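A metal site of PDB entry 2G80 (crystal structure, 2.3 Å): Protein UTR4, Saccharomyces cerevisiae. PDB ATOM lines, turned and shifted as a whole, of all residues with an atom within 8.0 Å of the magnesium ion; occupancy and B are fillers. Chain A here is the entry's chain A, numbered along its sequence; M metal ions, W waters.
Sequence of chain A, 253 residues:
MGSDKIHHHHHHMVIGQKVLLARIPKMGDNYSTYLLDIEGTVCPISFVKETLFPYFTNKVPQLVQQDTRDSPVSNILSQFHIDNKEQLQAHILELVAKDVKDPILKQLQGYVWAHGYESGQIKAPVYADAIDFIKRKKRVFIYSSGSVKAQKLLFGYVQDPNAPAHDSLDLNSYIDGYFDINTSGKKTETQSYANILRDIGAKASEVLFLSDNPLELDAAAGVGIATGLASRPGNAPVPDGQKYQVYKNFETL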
ATOM      1  N   ASP A  37      -6.578   8.195   6.618  1.00  0.00           N
ATOM      2  CA  ASP A  37      -5.750   8.240   7.805  1.00  0.00           C
ATOM      3  C   ASP A  37      -6.420   9.286   8.753  1.00  0.00           C
ATOM      4  O   ASP A  37      -7.197  10.144   8.253  1.00  0.00           O
ATOM      5  CB  ASP A  37      -4.351   8.701   7.440  1.00  0.00           C
ATOM      6  CG  ASP A  37      -3.453   8.906   8.652  1.00  0.00           C
ATOM      7  OD1 ASP A  37      -3.500   8.057   9.588  1.00  0.00           O
ATOM      8  OD2 ASP A  37      -2.741   9.922   8.670  1.00  0.00           O
ATOM      9  N   ILE A  38      -6.150   9.209  10.064  1.00  0.00           N
ATOM     10  CA  ILE A  38      -6.681  10.202  11.031  1.00  0.00           C
ATOM     11  C   ILE A  38      -5.735  11.372  11.269  1.00  0.00           C
ATOM     12  O   ILE A  38      -6.015  12.493  10.840  1.00  0.00           O
ATOM     13  CB  ILE A  38      -7.091   9.567  12.408  1.00  0.00           C
ATOM     14  CG1 ILE A  38      -8.249   8.585  12.179  1.00  0.00           C
ATOM     15  CG2 ILE A  38      -7.572  10.703  13.412  1.00  0.00           C
ATOM     16  CD1 ILE A  38      -8.702   7.801  13.365  1.00  0.00           C
ATOM     17  N   GLU A  39      -4.618  11.087  11.943  1.00  0.00           N
ATOM     18  CA  GLU A  39      -3.717  12.109  12.489  1.00  0.00           C
ATOM     19  C   GLU A  39      -2.920  12.793  11.417  1.00  0.00           C
ATOM     20  O   GLU A  39      -2.251  12.136  10.661  1.00  0.00           O
ATOM     21  CB  GLU A  39      -2.796  11.506  13.574  1.00  0.00           C
ATOM     22  CG  GLU A  39      -3.539  10.716  14.719  1.00  0.00           C
ATOM     23  CD  GLU A  39      -3.758   9.182  14.482  1.00  0.00           C
ATOM     24  OE1 GLU A  39      -3.845   8.681  13.311  1.00  0.00           O
ATOM     25  OE2 GLU A  39      -3.845   8.454  15.511  1.00  0.00           O
ATOM     26  N   GLY A  40      -2.996  14.121  11.323  1.00  0.00           N
ATOM     27  CA  GLY A  40      -2.337  14.867  10.231  1.00  0.00           C
ATOM     28  C   GLY A  40      -3.102  14.832   8.903  1.00  0.00           C
ATOM     29  O   GLY A  40      -2.671  15.437   7.910  1.00  0.00           O
ATOM     30  N   THR A  41      -4.258  14.150   8.884  1.00  0.00           N
ATOM     31  CA  THR A  41      -5.073  13.997   7.677  1.00  0.00           C
ATOM     32  C   THR A  41      -6.467  14.603   7.895  1.00  0.00           C
ATOM     33  O   THR A  41      -6.840  15.492   7.171  1.00  0.00           O
ATOM     34  CB  THR A  41      -5.093  12.516   7.275  1.00  0.00           C
ATOM     35  OG1 THR A  41      -3.746  12.088   7.055  1.00  0.00           O
ATOM     36  CG2 THR A  41      -5.886  12.300   6.005  1.00  0.00           C
ATOM     37  N   VAL A  42      -7.252  14.068   8.829  1.00  0.00           N
ATOM     38  CA  VAL A  42      -8.569  14.636   9.179  1.00  0.00           C
ATOM     39  C   VAL A  42      -8.563  15.390  10.533  1.00  0.00           C
ATOM     40  O   VAL A  42      -9.468  16.203  10.783  1.00  0.00           O
ATOM     41  CB  VAL A  42      -9.742  13.559   9.107  1.00  0.00           C
ATOM     42  CG1 VAL A  42      -9.743  12.816   7.760  1.00  0.00           C
ATOM     43  CG2 VAL A  42      -9.727  12.599  10.216  1.00  0.00           C
ATOM     44  N   CYS A  43      -7.546  15.124  11.377  1.00  0.00           N
ATOM     45  CA  CYS A  43      -7.406  15.747  12.703  1.00  0.00           C
ATOM     46  C   CYS A  43      -5.982  16.329  12.844  1.00  0.00           C
ATOM     47  O   CYS A  43      -5.019  15.727  12.307  1.00  0.00           O
ATOM     48  CB  CYS A  43      -7.648  14.678  13.786  1.00  0.00           C
ATOM     49  SG  CYS A  43      -7.729  15.248  15.510  1.00  0.00           S
ATOM     50  N   ILE A  45      -2.432  16.938  14.112  1.00  0.00           N
ATOM     51  CA  ILE A  45      -1.455  16.054  14.708  1.00  0.00           C
ATOM     52  C   ILE A  45      -1.194  16.474  16.181  1.00  0.00           C
ATOM     53  O   ILE A  45      -0.878  15.639  17.012  1.00  0.00           O
ATOM     54  CB  ILE A  45      -0.197  16.013  13.746  1.00  0.00           C
ATOM     55  CG1 ILE A  45       0.572  14.712  13.845  1.00  0.00           C
ATOM     56  CG2 ILE A  45       0.669  17.242  13.921  1.00  0.00           C
ATOM     57  CD1 ILE A  45       1.463  14.513  12.613  1.00  0.00           C
ATOM     58  N   TYR A 143      -8.550   4.164   8.560  1.00  0.00           N
ATOM     59  CA  TYR A 143      -7.420   3.293   8.905  1.00  0.00           C
ATOM     60  C   TYR A 143      -6.447   4.085   9.769  1.00  0.00           C
ATOM     61  O   TYR A 143      -5.883   5.077   9.296  1.00  0.00           O
ATOM     62  CB  TYR A 143      -6.703   2.755   7.669  1.00  0.00           C
ATOM     63  CG  TYR A 143      -5.565   1.738   7.873  1.00  0.00           C
ATOM     64  CD1 TYR A 143      -5.565   0.814   8.941  1.00  0.00           C
ATOM     65  CD2 TYR A 143      -4.555   1.611   6.913  1.00  0.00           C
ATOM     66  CE1 TYR A 143      -4.539  -0.150   9.089  1.00  0.00           C
ATOM     67  CE2 TYR A 143      -3.559   0.636   7.032  1.00  0.00           C
ATOM     68  CZ  TYR A 143      -3.552  -0.235   8.114  1.00  0.00           C
ATOM     69  OH  TYR A 143      -2.545  -1.145   8.209  1.00  0.00           O
ATOM     70  N   SER A 144      -6.240   3.647  11.015  1.00  0.00           N
ATOM     71  CA  SER A 144      -5.379   4.365  11.975  1.00  0.00           C
ATOM     72  C   SER A 144      -4.592   3.436  12.916  1.00  0.00           C
ATOM     73  O   SER A 144      -4.924   2.278  13.029  1.00  0.00           O
ATOM     74  CB  SER A 144      -6.258   5.322  12.809  1.00  0.00           C
ATOM     75  OG  SER A 144      -5.481   6.179  13.629  1.00  0.00           O
ATOM     76  N   SER A 145      -3.567   3.957  13.593  1.00  0.00           N
ATOM     77  CA  SER A 145      -2.811   3.200  14.627  1.00  0.00           C
ATOM     78  C   SER A 145      -3.683   3.005  15.889  1.00  0.00           C
ATOM     79  O   SER A 145      -3.531   2.006  16.610  1.00  0.00           O
ATOM     80  CB  SER A 145      -1.491   3.884  15.003  1.00  0.00           C
ATOM     81  OG  SER A 145      -1.706   5.202  15.499  1.00  0.00           O
ATOM     82  N   LYS A 187       0.728  -0.258   9.063  1.00  0.00           N
ATOM     83  CA  LYS A 187       0.372   0.765   8.050  1.00  0.00           C
ATOM     84  C   LYS A 187       1.355   0.945   6.889  1.00  0.00           C
ATOM     85  O   LYS A 187       0.976   1.530   5.865  1.00  0.00           O
ATOM     86  CB  LYS A 187       0.113   2.115   8.708  1.00  0.00           C
ATOM     87  CG  LYS A 187      -1.046   2.116   9.674  1.00  0.00           C
ATOM     88  CD  LYS A 187      -1.490   3.501  10.110  1.00  0.00           C
ATOM     89  CE  LYS A 187      -2.388   4.169   9.063  1.00  0.00           C
ATOM     90  NZ  LYS A 187      -2.722   5.576   9.398  1.00  0.00           N
ATOM     91  N   LEU A 210      -5.870   8.627   1.513  1.00  0.00           N
ATOM     92  CA  LEU A 210      -5.339   9.922   1.919  1.00  0.00           C
ATOM     93  C   LEU A 210      -4.629   9.784   3.274  1.00  0.00           C
ATOM     94  O   LEU A 210      -5.198   9.306   4.264  1.00  0.00           O
ATOM     95  CB  LEU A 210      -6.450  10.964   2.009  1.00  0.00           C
ATOM     96  CG  LEU A 210      -7.218  11.208   0.700  1.00  0.00           C
ATOM     97  CD1 LEU A 210      -8.594  11.833   0.985  1.00  0.00           C
ATOM     98  CD2 LEU A 210      -6.409  12.013  -0.311  1.00  0.00           C
ATOM     99  N   SER A 211      -3.370  10.221   3.293  1.00  0.00           N
ATOM    100  CA  SER A 211      -2.537  10.161   4.465  1.00  0.00           C
ATOM    101  C   SER A 211      -1.442  11.208   4.365  1.00  0.00           C
ATOM    102  O   SER A 211      -1.126  11.635   3.272  1.00  0.00           O
ATOM    103  CB  SER A 211      -1.960   8.738   4.617  1.00  0.00           C
ATOM    104  OG  SER A 211      -0.951   8.653   5.633  1.00  0.00           O
ATOM    105  N   ASP A 212      -0.933  11.661   5.520  1.00  0.00           N
ATOM    106  CA  ASP A 212       0.205  12.559   5.595  1.00  0.00           C
ATOM    107  C   ASP A 212       1.553  11.827   5.569  1.00  0.00           C
ATOM    108  O   ASP A 212       2.572  12.475   5.415  1.00  0.00           O
ATOM    109  CB  ASP A 212       0.158  13.473   6.836  1.00  0.00           C
ATOM    110  CG  ASP A 212       0.095  12.706   8.132  1.00  0.00           C
ATOM    111  OD1 ASP A 212      -0.585  11.650   8.146  1.00  0.00           O
ATOM    112  OD2 ASP A 212       0.697  13.154   9.141  1.00  0.00           O
ATOM    113  N   ASN A 213       1.540  10.496   5.714  1.00  0.00           N
ATOM    114  CA  ASN A 213       2.754   9.677   5.750  1.00  0.00           C
ATOM    115  C   ASN A 213       3.010   9.024   4.374  1.00  0.00           C
ATOM    116  O   ASN A 213       2.260   8.131   3.971  1.00  0.00           O
ATOM    117  CB  ASN A 213       2.603   8.612   6.850  1.00  0.00           C
ATOM    118  CG  ASN A 213       3.900   7.837   7.146  1.00  0.00           C
ATOM    119  OD1 ASN A 213       4.906   7.977   6.439  1.00  0.00           O
ATOM    120  ND2 ASN A 213       3.871   7.023   8.185  1.00  0.00           N
ATOM    121  N   GLU A 216       3.089   5.143   4.140  1.00  0.00           N
ATOM    122  CA  GLU A 216       1.785   4.509   4.131  1.00  0.00           C
ATOM    123  C   GLU A 216       1.278   4.486   2.677  1.00  0.00           C
ATOM    124  O   GLU A 216       0.795   3.473   2.214  1.00  0.00           O
ATOM    125  CB  GLU A 216       0.791   5.257   5.042  1.00  0.00           C
ATOM    126  CG  GLU A 216       1.182   5.227   6.534  1.00  0.00           C
ATOM    127  CD  GLU A 216       0.180   5.939   7.464  1.00  0.00           C
ATOM    128  OE1 GLU A 216      -0.860   6.472   6.986  1.00  0.00           O
ATOM    129  OE2 GLU A 216       0.429   5.951   8.686  1.00  0.00           O
ATOM    130  N   ALA A 230      -1.828  14.199   2.228  1.00  0.00           N
ATOM    131  CA  ALA A 230      -2.521  15.227   2.995  1.00  0.00           C
ATOM    132  C   ALA A 230      -1.472  16.166   3.627  1.00  0.00           C
ATOM    133  O   ALA A 230      -0.479  15.705   4.204  1.00  0.00           O
ATOM    134  CB  ALA A 230      -3.439  14.619   4.071  1.00  0.00           C
ATOM    135  N   ASN A 235       1.917  19.613  10.286  1.00  0.00           N
ATOM    136  CA  ASN A 235       2.534  18.358   9.760  1.00  0.00           C
ATOM    137  C   ASN A 235       4.011  18.620   9.418  1.00  0.00           C
ATOM    138  O   ASN A 235       4.432  19.759   9.243  1.00  0.00           O
ATOM    139  CB  ASN A 235       1.864  17.849   8.461  1.00  0.00           C
ATOM    140  CG  ASN A 235       0.470  17.289   8.659  1.00  0.00           C
ATOM    141  OD1 ASN A 235      -0.122  17.328   9.736  1.00  0.00           O
ATOM    142  ND2 ASN A 235      -0.073  16.751   7.579  1.00  0.00           N
HETATM  143 MG    MG M   1      -1.068  10.516   9.906  1.00  0.00          MG
HETATM  144  O   HOH W   1       0.513  11.148  10.878  1.00  0.00           O
HETATM  145  O   HOH W   2      -1.645   9.207  11.287  1.00  0.00           O
HETATM  146  O   HOH W   3      -0.158   8.880   8.997  1.00  0.00           O
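Water W2 bridges OD1 of Asp 37 (2.8 Å) and OE1 of Glu 39 (3.0 Å).
Water W3 lies within hydrogen-bond range of the side-chain carboxylate of Glu 216 (3.0 Å), the side-chain hydroxyl of Ser 211 (3.5 Å) and the side-chain carboxylate of Asp 37 (3.5 Å).
The magnesium ion is bound by water W1 (2.0 Å).
Water W2 binds the magnesium ion (2.0 Å).
The magnesium ion is bound by water W3 (2.1 Å).
The magnesium ion is bound by the backbone carbonyl oxygen (O) of Glu 39 (2.1 Å).
OD1 of Asp 212 is bound to the magnesium ion, at 2.1 Å.
The magnesium ion is bound by OD2 of Asp 37, at 2.2 Å.
The magnesium ion has six donor atoms within binding distance.
Three residues have an atom within 4 Å of the magnesium ion: Asp 37, Glu 39 and Asp 212.
The nearest printed residue that does not touch the magnesium ion is Thr 41 (4.2 Å).
N of Asp 37 lies within hydrogen-bond range of O of Leu 210 (2.9 Å).
N of Asp 212 is in hydrogen-bond range of OG1 of Thr 41 (3.2 Å).
The side-chain carboxylate of Glu 39 sits at hydrogen-bond distance from the side-chain hydroxyl of Ser 144, at 3.0 Å.
The side-chain amino group of Lys 187 lies within salt-bridge range of the side-chain carboxylate of Asp 37 (2.6 Å).
The side-chain hydroxyl of Thr 41 lies close to the side-chain carboxylate of Asp 37, 2.9 Å away.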
